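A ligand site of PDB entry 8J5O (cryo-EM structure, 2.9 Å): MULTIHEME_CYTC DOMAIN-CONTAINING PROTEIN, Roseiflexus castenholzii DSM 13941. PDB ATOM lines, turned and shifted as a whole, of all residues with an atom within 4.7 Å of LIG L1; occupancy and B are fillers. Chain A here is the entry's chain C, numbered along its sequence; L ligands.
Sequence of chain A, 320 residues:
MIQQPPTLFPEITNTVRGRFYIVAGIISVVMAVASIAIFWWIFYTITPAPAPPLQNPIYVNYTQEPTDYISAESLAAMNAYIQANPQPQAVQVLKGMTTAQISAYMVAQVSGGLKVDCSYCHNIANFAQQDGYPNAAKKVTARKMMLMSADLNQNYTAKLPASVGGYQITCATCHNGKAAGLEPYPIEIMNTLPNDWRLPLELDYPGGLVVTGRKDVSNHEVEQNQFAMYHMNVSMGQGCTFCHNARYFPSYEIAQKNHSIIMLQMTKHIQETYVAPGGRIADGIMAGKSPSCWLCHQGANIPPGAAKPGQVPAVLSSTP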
ATOM      1  N   MET A  78      -4.623 -22.947 -14.652  1.00  0.00           N
ATOM      2  CA  MET A  78      -4.887 -21.935 -13.636  1.00  0.00           C
ATOM      3  C   MET A  78      -5.109 -20.570 -14.266  1.00  0.00           C
ATOM      4  O   MET A  78      -6.077 -19.867 -13.934  1.00  0.00           O
ATOM      5  CB  MET A  78      -3.702 -21.881 -12.669  1.00  0.00           C
ATOM      6  CG  MET A  78      -3.982 -21.283 -11.314  1.00  0.00           C
ATOM      7  SD  MET A  78      -2.746 -21.929 -10.163  1.00  0.00           S
ATOM      8  CE  MET A  78      -3.105 -23.688 -10.192  1.00  0.00           C
ATOM      9  N   TYR A  81      -8.423 -20.350 -16.235  1.00  0.00           N
ATOM     10  CA  TYR A  81      -9.558 -20.170 -15.330  1.00  0.00           C
ATOM     11  C   TYR A  81      -9.622 -18.757 -14.824  1.00  0.00           C
ATOM     12  O   TYR A  81     -10.674 -18.131 -14.833  1.00  0.00           O
ATOM     13  CB  TYR A  81      -9.502 -21.116 -14.131  1.00  0.00           C
ATOM     14  CG  TYR A  81     -10.835 -21.187 -13.417  1.00  0.00           C
ATOM     15  CD1 TYR A  81     -11.889 -21.863 -13.980  1.00  0.00           C
ATOM     16  CD2 TYR A  81     -11.031 -20.555 -12.197  1.00  0.00           C
ATOM     17  CE1 TYR A  81     -13.113 -21.935 -13.361  1.00  0.00           C
ATOM     18  CE2 TYR A  81     -12.256 -20.613 -11.567  1.00  0.00           C
ATOM     19  CZ  TYR A  81     -13.298 -21.305 -12.156  1.00  0.00           C
ATOM     20  OH  TYR A  81     -14.525 -21.372 -11.553  1.00  0.00           O
ATOM     21  N   PRO A  88     -14.756 -15.235  -8.038  1.00  0.00           N
ATOM     22  CA  PRO A  88     -15.021 -16.647  -7.756  1.00  0.00           C
ATOM     23  C   PRO A  88     -16.505 -16.967  -7.889  1.00  0.00           C
ATOM     24  O   PRO A  88     -17.367 -16.110  -7.668  1.00  0.00           O
ATOM     25  CB  PRO A  88     -14.535 -16.824  -6.325  1.00  0.00           C
ATOM     26  CG  PRO A  88     -14.669 -15.476  -5.721  1.00  0.00           C
ATOM     27  CD  PRO A  88     -14.362 -14.496  -6.827  1.00  0.00           C
ATOM     28  N   GLN A  89     -16.789 -18.214  -8.252  1.00  0.00           N
ATOM     29  CA  GLN A  89     -18.151 -18.695  -8.385  1.00  0.00           C
ATOM     30  C   GLN A  89     -18.312 -19.991  -7.597  1.00  0.00           C
ATOM     31  O   GLN A  89     -17.443 -20.862  -7.640  1.00  0.00           O
ATOM     32  CB  GLN A  89     -18.522 -18.928  -9.855  1.00  0.00           C
ATOM     33  CG  GLN A  89     -17.481 -19.714 -10.632  1.00  0.00           C
ATOM     34  CD  GLN A  89     -17.604 -19.512 -12.125  1.00  0.00           C
ATOM     35  OE1 GLN A  89     -17.968 -20.419 -12.865  1.00  0.00           O
ATOM     36  NE2 GLN A  89     -17.301 -18.300 -12.574  1.00  0.00           N
ATOM     37  N   ALA A  90     -19.431 -20.098  -6.885  1.00  0.00           N
ATOM     38  CA  ALA A  90     -19.733 -21.285  -6.076  1.00  0.00           C
ATOM     39  C   ALA A  90     -18.738 -21.430  -4.927  1.00  0.00           C
ATOM     40  O   ALA A  90     -18.240 -22.522  -4.657  1.00  0.00           O
ATOM     41  CB  ALA A  90     -19.771 -22.544  -6.928  1.00  0.00           C
ATOM     42  N   VAL A  91     -18.446 -20.320  -4.245  1.00  0.00           N
ATOM     43  CA  VAL A  91     -17.589 -20.320  -3.066  1.00  0.00           C
ATOM     44  C   VAL A  91     -18.469 -20.123  -1.839  1.00  0.00           C
ATOM     45  O   VAL A  91     -19.363 -19.272  -1.839  1.00  0.00           O
ATOM     46  CB  VAL A  91     -16.510 -19.230  -3.159  1.00  0.00           C
ATOM     47  CG1 VAL A  91     -17.136 -17.845  -3.158  1.00  0.00           C
ATOM     48  CG2 VAL A  91     -15.518 -19.370  -2.027  1.00  0.00           C
ATOM     49  N   GLN A  92     -18.219 -20.915  -0.797  1.00  0.00           N
ATOM     50  CA  GLN A  92     -19.052 -20.892   0.396  1.00  0.00           C
ATOM     51  C   GLN A  92     -18.329 -20.409   1.651  1.00  0.00           C
ATOM     52  O   GLN A  92     -19.008 -20.094   2.642  1.00  0.00           O
ATOM     53  CB  GLN A  92     -19.630 -22.290   0.668  1.00  0.00           C
ATOM     54  CG  GLN A  92     -20.506 -22.817  -0.441  1.00  0.00           C
ATOM     55  CD  GLN A  92     -20.736 -24.314  -0.336  1.00  0.00           C
ATOM     56  OE1 GLN A  92     -20.940 -24.855   0.745  1.00  0.00           O
ATOM     57  NE2 GLN A  92     -20.695 -24.992  -1.479  1.00  0.00           N
ATOM     58  N   VAL A  93     -17.010 -20.348   1.644  1.00  0.00           N
ATOM     59  CA  VAL A  93     -16.259 -19.937   2.830  1.00  0.00           C
ATOM     60  C   VAL A  93     -15.398 -18.722   2.496  1.00  0.00           C
ATOM     61  O   VAL A  93     -15.544 -17.654   3.104  1.00  0.00           O
ATOM     62  CB  VAL A  93     -15.387 -21.081   3.375  1.00  0.00           C
ATOM     63  CG1 VAL A  93     -14.347 -20.540   4.342  1.00  0.00           C
ATOM     64  CG2 VAL A  93     -16.263 -22.118   4.054  1.00  0.00           C
ATOM     65  N   LEU A  94     -14.510 -18.867   1.514  1.00  0.00           N
ATOM     66  CA  LEU A  94     -13.593 -17.795   1.135  1.00  0.00           C
ATOM     67  C   LEU A  94     -14.391 -16.673   0.485  1.00  0.00           C
ATOM     68  O   LEU A  94     -14.805 -16.779  -0.679  1.00  0.00           O
ATOM     69  CB  LEU A  94     -12.516 -18.330   0.196  1.00  0.00           C
ATOM     70  CG  LEU A  94     -11.618 -19.428   0.767  1.00  0.00           C
ATOM     71  CD1 LEU A  94     -10.679 -19.950  -0.313  1.00  0.00           C
ATOM     72  CD2 LEU A  94     -10.841 -18.921   1.969  1.00  0.00           C
ATOM     73  N   THR A  99     -10.486 -14.057  -7.662  1.00  0.00           N
ATOM     74  CA  THR A  99      -9.968 -15.344  -8.109  1.00  0.00           C
ATOM     75  C   THR A  99      -8.446 -15.405  -8.017  1.00  0.00           C
ATOM     76  O   THR A  99      -7.887 -16.457  -7.693  1.00  0.00           O
ATOM     77  CB  THR A  99     -10.434 -15.635  -9.541  1.00  0.00           C
ATOM     78  OG1 THR A  99     -11.866 -15.658  -9.581  1.00  0.00           O
ATOM     79  CG2 THR A  99      -9.905 -16.980 -10.006  1.00  0.00           C
ATOM     80  N   ILE A 102      -7.556 -15.916  -4.306  1.00  0.00           N
ATOM     81  CA  ILE A 102      -7.897 -17.269  -3.902  1.00  0.00           C
ATOM     82  C   ILE A 102      -6.919 -18.269  -4.483  1.00  0.00           C
ATOM     83  O   ILE A 102      -6.523 -19.237  -3.824  1.00  0.00           O
ATOM     84  CB  ILE A 102      -9.349 -17.600  -4.305  1.00  0.00           C
ATOM     85  CG1 ILE A 102     -10.338 -16.824  -3.432  1.00  0.00           C
ATOM     86  CG2 ILE A 102      -9.611 -19.094  -4.175  1.00  0.00           C
ATOM     87  CD1 ILE A 102     -11.782 -17.171  -3.695  1.00  0.00           C
ATOM     88  N   SER A 103      -6.510 -18.060  -5.739  1.00  0.00           N
ATOM     89  CA  SER A 103      -5.523 -18.954  -6.359  1.00  0.00           C
ATOM     90  C   SER A 103      -4.180 -18.861  -5.648  1.00  0.00           C
ATOM     91  O   SER A 103      -3.503 -19.870  -5.456  1.00  0.00           O
ATOM     92  CB  SER A 103      -5.375 -18.611  -7.839  1.00  0.00           C
ATOM     93  OG  SER A 103      -4.818 -17.324  -8.016  1.00  0.00           O
ATOM     94  N   MET A 106      -4.498 -20.791  -2.461  1.00  0.00           N
ATOM     95  CA  MET A 106      -4.474 -22.224  -2.721  1.00  0.00           C
ATOM     96  C   MET A 106      -3.071 -22.714  -3.038  1.00  0.00           C
ATOM     97  O   MET A 106      -2.652 -23.779  -2.551  1.00  0.00           O
ATOM     98  CB  MET A 106      -5.439 -22.553  -3.862  1.00  0.00           C
ATOM     99  CG  MET A 106      -6.899 -22.367  -3.521  1.00  0.00           C
ATOM    100  SD  MET A 106      -7.713 -23.865  -2.941  1.00  0.00           S
ATOM    101  CE  MET A 106      -8.953 -23.154  -1.867  1.00  0.00           C
ATOM    102  N   VAL A 107      -2.327 -21.970  -3.848  1.00  0.00           N
ATOM    103  CA  VAL A 107      -0.987 -22.386  -4.230  1.00  0.00           C
ATOM    104  C   VAL A 107      -0.046 -22.356  -3.040  1.00  0.00           C
ATOM    105  O   VAL A 107       0.734 -23.293  -2.817  1.00  0.00           O
ATOM    106  CB  VAL A 107      -0.451 -21.495  -5.380  1.00  0.00           C
ATOM    107  CG1 VAL A 107       0.981 -21.871  -5.695  1.00  0.00           C
ATOM    108  CG2 VAL A 107      -1.324 -21.644  -6.609  1.00  0.00           C
ATOM    109  N   VAL A 110      -2.860 -23.980   0.809  1.00  0.00           N
ATOM    110  CA  VAL A 110      -3.547 -25.264   0.749  1.00  0.00           C
ATOM    111  C   VAL A 110      -2.637 -26.338   0.178  1.00  0.00           C
ATOM    112  O   VAL A 110      -2.528 -27.438   0.733  1.00  0.00           O
ATOM    113  CB  VAL A 110      -4.848 -25.136  -0.060  1.00  0.00           C
ATOM    114  CG1 VAL A 110      -5.480 -26.498  -0.255  1.00  0.00           C
ATOM    115  CG2 VAL A 110      -5.811 -24.185   0.620  1.00  0.00           C
ATOM    116  N   SER A 111      -1.965 -26.041  -0.932  1.00  0.00           N
ATOM    117  CA  SER A 111      -1.048 -26.999  -1.545  1.00  0.00           C
ATOM    118  C   SER A 111       0.346 -26.960  -0.926  1.00  0.00           C
ATOM    119  O   SER A 111       1.015 -27.990  -0.853  1.00  0.00           O
ATOM    120  CB  SER A 111      -0.947 -26.758  -3.044  1.00  0.00           C
ATOM    121  OG  SER A 111      -2.190 -26.981  -3.689  1.00  0.00           O
ATOM    122  N   LEU A 114       0.183 -29.014   2.411  1.00  0.00           N
ATOM    123  CA  LEU A 114      -0.060 -30.448   2.299  1.00  0.00           C
ATOM    124  C   LEU A 114       0.837 -31.155   1.297  1.00  0.00           C
ATOM    125  O   LEU A 114       0.930 -32.387   1.342  1.00  0.00           O
ATOM    126  CB  LEU A 114      -1.531 -30.706   1.932  1.00  0.00           C
ATOM    127  CG  LEU A 114      -2.551 -30.695   3.066  1.00  0.00           C
ATOM    128  CD1 LEU A 114      -2.742 -29.302   3.615  1.00  0.00           C
ATOM    129  CD2 LEU A 114      -3.877 -31.279   2.605  1.00  0.00           C
ATOM    130  N   VAL A 116       0.514 -31.451  -2.101  1.00  0.00           N
ATOM    131  CA  VAL A 116      -0.324 -32.228  -2.990  1.00  0.00           C
ATOM    132  C   VAL A 116      -0.636 -31.409  -4.231  1.00  0.00           C
ATOM    133  O   VAL A 116      -0.529 -30.181  -4.242  1.00  0.00           O
ATOM    134  CB  VAL A 116      -1.638 -32.682  -2.308  1.00  0.00           C
ATOM    135  CG1 VAL A 116      -1.337 -33.602  -1.136  1.00  0.00           C
ATOM    136  CG2 VAL A 116      -2.447 -31.481  -1.861  1.00  0.00           C
ATOM    137  N   ASP A 117      -1.025 -32.116  -5.288  1.00  0.00           N
ATOM    138  CA  ASP A 117      -1.368 -31.483  -6.557  1.00  0.00           C
ATOM    139  C   ASP A 117      -2.766 -30.885  -6.491  1.00  0.00           C
ATOM    140  O   ASP A 117      -3.571 -31.196  -5.603  1.00  0.00           O
ATOM    141  CB  ASP A 117      -1.276 -32.485  -7.703  1.00  0.00           C
ATOM    142  CG  ASP A 117      -0.981 -31.828  -9.031  1.00  0.00           C
ATOM    143  OD1 ASP A 117      -0.105 -30.929  -9.072  1.00  0.00           O
ATOM    144  OD2 ASP A 117      -1.625 -32.190 -10.035  1.00  0.00           O
ATOM    145  N   CYS A 118      -3.065 -30.013  -7.457  1.00  0.00           N
ATOM    146  CA  CYS A 118      -4.371 -29.372  -7.506  1.00  0.00           C
ATOM    147  C   CYS A 118      -5.482 -30.378  -7.779  1.00  0.00           C
ATOM    148  O   CYS A 118      -6.625 -30.184  -7.338  1.00  0.00           O
ATOM    149  CB  CYS A 118      -4.384 -28.275  -8.567  1.00  0.00           C
ATOM    150  SG  CYS A 118      -3.591 -26.732  -8.053  1.00  0.00           S
ATOM    151  N   TYR A 120      -5.770 -33.223  -6.494  1.00  0.00           N
ATOM    152  CA  TYR A 120      -6.021 -34.052  -5.319  1.00  0.00           C
ATOM    153  C   TYR A 120      -7.422 -33.806  -4.772  1.00  0.00           C
ATOM    154  O   TYR A 120      -8.113 -34.751  -4.364  1.00  0.00           O
ATOM    155  CB  TYR A 120      -4.952 -33.787  -4.265  1.00  0.00           C
ATOM    156  CG  TYR A 120      -5.059 -34.622  -2.998  1.00  0.00           C
ATOM    157  CD1 TYR A 120      -5.876 -34.238  -1.949  1.00  0.00           C
ATOM    158  CD2 TYR A 120      -4.291 -35.769  -2.849  1.00  0.00           C
ATOM    159  CE1 TYR A 120      -5.969 -34.994  -0.803  1.00  0.00           C
ATOM    160  CE2 TYR A 120      -4.368 -36.532  -1.701  1.00  0.00           C
ATOM    161  CZ  TYR A 120      -5.211 -36.139  -0.676  1.00  0.00           C
ATOM    162  OH  TYR A 120      -5.290 -36.892   0.468  1.00  0.00           O
ATOM    163  N   CYS A 121      -7.851 -32.554  -4.730  1.00  0.00           N
ATOM    164  CA  CYS A 121      -9.109 -32.181  -4.077  1.00  0.00           C
ATOM    165  C   CYS A 121     -10.225 -31.921  -5.073  1.00  0.00           C
ATOM    166  O   CYS A 121     -11.328 -32.464  -4.931  1.00  0.00           O
ATOM    167  CB  CYS A 121      -8.888 -30.951  -3.188  1.00  0.00           C
ATOM    168  SG  CYS A 121      -8.129 -31.296  -1.582  1.00  0.00           S
ATOM    169  N   HIS A 122      -9.977 -31.090  -6.081  1.00  0.00           N
ATOM    170  CA  HIS A 122     -11.026 -30.635  -6.980  1.00  0.00           C
ATOM    171  C   HIS A 122     -10.526 -30.489  -8.411  1.00  0.00           C
ATOM    172  O   HIS A 122      -9.344 -30.210  -8.648  1.00  0.00           O
ATOM    173  CB  HIS A 122     -11.654 -29.338  -6.443  1.00  0.00           C
ATOM    174  CG  HIS A 122     -10.679 -28.197  -6.332  1.00  0.00           C
ATOM    175  ND1 HIS A 122     -10.404 -27.341  -7.375  1.00  0.00           N
ATOM    176  CD2 HIS A 122      -9.938 -27.761  -5.289  1.00  0.00           C
ATOM    177  CE1 HIS A 122      -9.528 -26.432  -6.974  1.00  0.00           C
ATOM    178  NE2 HIS A 122      -9.233 -26.670  -5.713  1.00  0.00           N
ATOM    179  N   PHE A 127     -12.792 -25.727 -12.041  1.00  0.00           N
ATOM    180  CA  PHE A 127     -12.430 -25.604 -10.636  1.00  0.00           C
ATOM    181  C   PHE A 127     -13.637 -25.423  -9.724  1.00  0.00           C
ATOM    182  O   PHE A 127     -13.495 -25.597  -8.508  1.00  0.00           O
ATOM    183  CB  PHE A 127     -11.461 -24.424 -10.471  1.00  0.00           C
ATOM    184  CG  PHE A 127     -10.028 -24.782 -10.763  1.00  0.00           C
ATOM    185  CD1 PHE A 127      -9.460 -25.899 -10.196  1.00  0.00           C
ATOM    186  CD2 PHE A 127      -9.249 -23.995 -11.591  1.00  0.00           C
ATOM    187  CE1 PHE A 127      -8.144 -26.237 -10.430  1.00  0.00           C
ATOM    188  CE2 PHE A 127      -7.936 -24.328 -11.842  1.00  0.00           C
ATOM    189  CZ  PHE A 127      -7.386 -25.456 -11.262  1.00  0.00           C
ATOM    190  N   ALA A 128     -14.804 -25.098 -10.278  1.00  0.00           N
ATOM    191  CA  ALA A 128     -16.011 -24.845  -9.497  1.00  0.00           C
ATOM    192  C   ALA A 128     -16.894 -26.075  -9.322  1.00  0.00           C
ATOM    193  O   ALA A 128     -17.931 -25.976  -8.647  1.00  0.00           O
ATOM    194  CB  ALA A 128     -16.830 -23.728 -10.150  1.00  0.00           C
ATOM    195  N   LYS A 139     -12.535 -32.397  -0.924  1.00  0.00           N
ATOM    196  CA  LYS A 139     -12.855 -30.975  -0.915  1.00  0.00           C
ATOM    197  C   LYS A 139     -13.803 -30.635   0.231  1.00  0.00           C
ATOM    198  O   LYS A 139     -13.663 -29.571   0.862  1.00  0.00           O
ATOM    199  CB  LYS A 139     -13.453 -30.564  -2.260  1.00  0.00           C
ATOM    200  CG  LYS A 139     -13.734 -29.082  -2.412  1.00  0.00           C
ATOM    201  CD  LYS A 139     -14.241 -28.773  -3.821  1.00  0.00           C
ATOM    202  CE  LYS A 139     -14.523 -27.295  -3.987  1.00  0.00           C
ATOM    203  NZ  LYS A 139     -15.032 -26.984  -5.358  1.00  0.00           N
ATOM    204  N   ALA A 142     -11.751 -30.532   3.248  1.00  0.00           N
ATOM    205  CA  ALA A 142     -10.956 -29.298   3.261  1.00  0.00           C
ATOM    206  C   ALA A 142     -11.783 -28.106   3.721  1.00  0.00           C
ATOM    207  O   ALA A 142     -11.281 -27.248   4.465  1.00  0.00           O
ATOM    208  CB  ALA A 142     -10.371 -29.048   1.868  1.00  0.00           C
ATOM    209  N   ARG A 143     -13.031 -28.017   3.275  1.00  0.00           N
ATOM    210  CA  ARG A 143     -13.895 -26.929   3.738  1.00  0.00           C
ATOM    211  C   ARG A 143     -14.140 -27.016   5.235  1.00  0.00           C
ATOM    212  O   ARG A 143     -14.117 -26.008   5.952  1.00  0.00           O
ATOM    213  CB  ARG A 143     -15.214 -26.942   2.966  1.00  0.00           C
ATOM    214  CG  ARG A 143     -16.137 -25.782   3.289  1.00  0.00           C
ATOM    215  CD  ARG A 143     -17.409 -25.838   2.459  1.00  0.00           C
ATOM    216  NE  ARG A 143     -17.140 -25.690   1.036  1.00  0.00           N
ATOM    217  CZ  ARG A 143     -17.305 -26.644   0.141  1.00  0.00           C
ATOM    218  NH1 ARG A 143     -17.735 -27.845   0.471  1.00  0.00           N
ATOM    219  NH2 ARG A 143     -17.036 -26.381  -1.134  1.00  0.00           N
ATOM    220  N   MET A 146     -11.093 -25.790   6.965  1.00  0.00           N
ATOM    221  CA  MET A 146     -11.022 -24.328   6.972  1.00  0.00           C
ATOM    222  C   MET A 146     -11.922 -23.727   8.042  1.00  0.00           C
ATOM    223  O   MET A 146     -11.530 -22.794   8.747  1.00  0.00           O
ATOM    224  CB  MET A 146     -11.391 -23.780   5.592  1.00  0.00           C
ATOM    225  CG  MET A 146     -10.475 -24.235   4.468  1.00  0.00           C
ATOM    226  SD  MET A 146     -10.736 -23.293   2.960  1.00  0.00           S
ATOM    227  CE  MET A 146     -10.381 -24.534   1.722  1.00  0.00           C
HETATM  228  C1  LIG L   1     -11.900 -23.691  -4.087  1.00  0.00           C
HETATM  229  C2  LIG L   1      -7.898 -23.057  -6.732  1.00  0.00           C
HETATM  230  C3  LIG L   1      -5.939 -26.991  -4.732  1.00  0.00           C
HETATM  231  C4  LIG L   1      -9.594 -27.122  -1.585  1.00  0.00           C
HETATM  232  C5  LIG L   1     -11.010 -23.225  -5.039  1.00  0.00           C
HETATM  233  C6  LIG L   1     -11.289 -22.222  -6.039  1.00  0.00           C
HETATM  234  C7  LIG L   1     -10.189 -22.048  -6.766  1.00  0.00           C
HETATM  235  C8  LIG L   1      -9.169 -22.938  -6.251  1.00  0.00           C
HETATM  236  C9  LIG L   1      -9.994 -21.071  -7.949  1.00  0.00           C
HETATM  237  C10 LIG L   1     -12.635 -21.482  -6.217  1.00  0.00           C
HETATM  238  C11 LIG L   1     -13.157 -21.712  -7.628  1.00  0.00           C
HETATM  239  C12 LIG L   1     -14.399 -20.898  -7.866  1.00  0.00           C
HETATM  240  O1  LIG L   1     -14.889 -20.866  -9.026  1.00  0.00           O
HETATM  241  O2  LIG L   1     -14.906 -20.278  -6.895  1.00  0.00           O
HETATM  242  C13 LIG L   1      -7.024 -24.048  -6.371  1.00  0.00           C
HETATM  243  C14 LIG L   1      -5.660 -24.129  -6.822  1.00  0.00           C
HETATM  244  C15 LIG L   1      -5.099 -25.210  -6.268  1.00  0.00           C
HETATM  245  C16 LIG L   1      -6.109 -25.853  -5.459  1.00  0.00           C
HETATM  246  C17 LIG L   1      -5.047 -23.073  -7.745  1.00  0.00           C
HETATM  247  C18 LIG L   1      -3.661 -25.764  -6.415  1.00  0.00           C
HETATM  248  C19 LIG L   1      -2.710 -24.995  -5.837  1.00  0.00           C
HETATM  249  C20 LIG L   1      -6.764 -27.375  -3.702  1.00  0.00           C
HETATM  250  C21 LIG L   1      -6.559 -28.529  -2.852  1.00  0.00           C
HETATM  251  C22 LIG L   1      -7.577 -28.563  -1.980  1.00  0.00           C
HETATM  252  C23 LIG L   1      -8.445 -27.430  -2.272  1.00  0.00           C
HETATM  253  C24 LIG L   1      -5.363 -29.505  -2.974  1.00  0.00           C
HETATM  254  C25 LIG L   1      -7.883 -29.566  -0.844  1.00  0.00           C
HETATM  255  C26 LIG L   1      -7.321 -29.227   0.357  1.00  0.00           C
HETATM  256  C27 LIG L   1     -10.537 -26.216  -2.000  1.00  0.00           C
HETATM  257  C28 LIG L   1     -11.805 -25.987  -1.354  1.00  0.00           C
HETATM  258  C29 LIG L   1     -12.447 -25.041  -2.040  1.00  0.00           C
HETATM  259  C30 LIG L   1     -11.601 -24.636  -3.147  1.00  0.00           C
HETATM  260  C31 LIG L   1     -12.327 -26.699  -0.096  1.00  0.00           C
HETATM  261  C32 LIG L   1     -13.845 -24.471  -1.708  1.00  0.00           C
HETATM  262  C33 LIG L   1     -13.666 -23.095  -1.063  1.00  0.00           C
HETATM  263  C34 LIG L   1     -14.989 -22.574  -0.569  1.00  0.00           C
HETATM  264  O3  LIG L   1     -15.002 -21.516   0.096  1.00  0.00           O
HETATM  265  O4  LIG L   1     -16.025 -23.225  -0.848  1.00  0.00           O
HETATM  266  N1  LIG L   1      -9.698 -23.655  -5.194  1.00  0.00           N
HETATM  267  N2  LIG L   1      -7.274 -25.108  -5.530  1.00  0.00           N
HETATM  268  N3  LIG L   1      -7.922 -26.716  -3.335  1.00  0.00           N
HETATM  269  N4  LIG L   1     -10.438 -25.387  -3.090  1.00  0.00           N
HETATM  270 FE1  LIG L   1      -8.816 -25.175  -4.245  1.00  0.00          FE
HETATM  271  C1  LG2 L   2      -7.108 -34.358   7.453  1.00  0.00           C
HETATM  272  C2  LG2 L   2      -7.108 -30.388   4.642  1.00  0.00           C
HETATM  273  C3  LG2 L   2      -5.991 -27.717   8.544  1.00  0.00           C
HETATM  274  C4  LG2 L   2      -5.561 -31.722  11.203  1.00  0.00           C
HETATM  275  C5  LG2 L   2      -7.240 -33.512   6.380  1.00  0.00           C
HETATM  276  C6  LG2 L   2      -7.700 -33.883   5.059  1.00  0.00           C
HETATM  277  C7  LG2 L   2      -7.687 -32.799   4.294  1.00  0.00           C
HETATM  278  C8  LG2 L   2      -7.230 -31.689   5.110  1.00  0.00           C
HETATM  279  C9  LG2 L   2      -8.095 -32.721   2.815  1.00  0.00           C
HETATM  280  C10 LG2 L   2      -8.115 -35.286   4.592  1.00  0.00           C
HETATM  281  C11 LG2 L   2      -6.943 -36.250   4.709  1.00  0.00           C
HETATM  282  C12 LG2 L   2      -7.250 -37.489   3.908  1.00  0.00           C
HETATM  283  O1  LG2 L   2      -6.405 -38.411   3.855  1.00  0.00           O
HETATM  284  O2  LG2 L   2      -8.363 -37.553   3.314  1.00  0.00           O
HETATM  285  C13 LG2 L   2      -6.777 -29.335   5.484  1.00  0.00           C
HETATM  286  C14 LG2 L   2      -6.640 -27.959   5.039  1.00  0.00           C
HETATM  287  C15 LG2 L   2      -6.346 -27.219   6.118  1.00  0.00           C
HETATM  288  C16 LG2 L   2      -6.277 -28.105   7.264  1.00  0.00           C
HETATM  289  C17 LG2 L   2      -6.829 -27.503   3.576  1.00  0.00           C
HETATM  290  C18 LG2 L   2      -6.082 -25.690   6.216  1.00  0.00           C
HETATM  291  C19 LG2 L   2      -7.121 -24.955   6.680  1.00  0.00           C
HETATM  292  C20 LG2 L   2      -5.749 -28.574   9.617  1.00  0.00           C
HETATM  293  C21 LG2 L   2      -5.353 -28.178  10.921  1.00  0.00           C
HETATM  294  C22 LG2 L   2      -5.229 -29.289  11.659  1.00  0.00           C
HETATM  295  C23 LG2 L   2      -5.567 -30.409  10.811  1.00  0.00           C
HETATM  296  C24 LG2 L   2      -5.119 -26.706  11.345  1.00  0.00           C
HETATM  297  C25 LG2 L   2      -4.823 -29.449  13.152  1.00  0.00           C
HETATM  298  C26 LG2 L   2      -5.894 -29.451  13.988  1.00  0.00           C
HETATM  299  C27 LG2 L   2      -5.928 -32.776  10.410  1.00  0.00           C
HETATM  300  C28 LG2 L   2      -5.918 -34.172  10.809  1.00  0.00           C
HETATM  301  C29 LG2 L   2      -6.346 -34.891   9.774  1.00  0.00           C
HETATM  302  C30 LG2 L   2      -6.645 -33.995   8.686  1.00  0.00           C
HETATM  303  C31 LG2 L   2      -5.492 -34.722  12.183  1.00  0.00           C
HETATM  304  C32 LG2 L   2      -6.489 -36.426   9.749  1.00  0.00           C
HETATM  305  C33 LG2 L   2      -5.503 -37.000   8.743  1.00  0.00           C
HETATM  306  C34 LG2 L   2      -5.470 -38.496   8.866  1.00  0.00           C
HETATM  307  O3  LG2 L   2      -4.533 -39.124   8.299  1.00  0.00           O
HETATM  308  O4  LG2 L   2      -6.367 -39.070   9.533  1.00  0.00           O
HETATM  309  N1  LG2 L   2      -7.021 -32.106   6.362  1.00  0.00           N
HETATM  310  N2  LG2 L   2      -6.548 -29.388   6.852  1.00  0.00           N
HETATM  311  N3  LG2 L   2      -5.883 -29.949   9.555  1.00  0.00           N
HETATM  312  N4  LG2 L   2      -6.383 -32.693   9.100  1.00  0.00           N
HETATM  313 FE1  LG2 L   2      -6.443 -31.047   7.976  1.00  0.00          FE
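The side-chain sulfur (SG) of Cys 121 is bonded to a carbon (C25) of LIG L1 (1.9 Å).
SG of Cys 118 is covalently linked to C18 of LIG L1 (1.9 Å).
NE2 of His 122 binds FE1 of LIG L1 (2.1 Å).
An iron atom (FE1) of LIG L1 is bound by the side-chain sulfur (SD) of Met 106.
An oxygen (O1) of LIG L1 is in hydrogen-bond range of the side-chain hydroxyl of Tyr 81, 2.6 Å away.
An oxygen (O2) of LIG L1 sits at hydrogen-bond distance from the backbone NH (N) of Gln 89, at 3.1 Å.
O2 of LIG L1 sits close to O of Gln 89, 2.7 Å away.
N of Val 93 lies within hydrogen-bond range of O3 of LIG L1, at 2.8 Å.
The backbone NH of Leu 94 lies within hydrogen-bond range of an oxygen (O3) of LIG L1.
An oxygen (O4) of LIG L1 sits at hydrogen-bond distance from the backbone NH of Gln 92.
The guanidinium group (NE) of Arg 143 is in salt-bridge range of an oxygen (O4) of LIG L1 (3.3 Å).
O of Met 106 is in hydrogen-bond range of N of Ser 111.
Merely in contact with LIG L1: Met 78 (3.2 Å), Pro 88 (3.5 Å), Val 91 (3.1 Å), Ile 102 (3.97 Å), Val 107 (3.5 Å), Val 110 (3.3 Å), Ser 111 (3.0 Å), Val 116 (3.7 Å), Asp 117 (3.6 Å), Phe 127 (3.998 Å), Ala 128 (3.6 Å), Lys 139 (3.3 Å), Ala 142 (3.4 Å) and Met 146 (3.4 Å).
Within 4 Å of LIG L1: Met 78, Tyr 81, Pro 88, Gln 89, Val 91, Gln 92, Val 93, Leu 94, Ile 102, Met 106, Val 107, Val 110, Ser 111, Val 116, Asp 117, Cys 118, Cys 121, His 122, Phe 127, Ala 128, Lys 139, Ala 142, Arg 143 and Met 146.
The nearest printed residue that does not touch LIG L1 is Ser 103 (4.2 Å).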
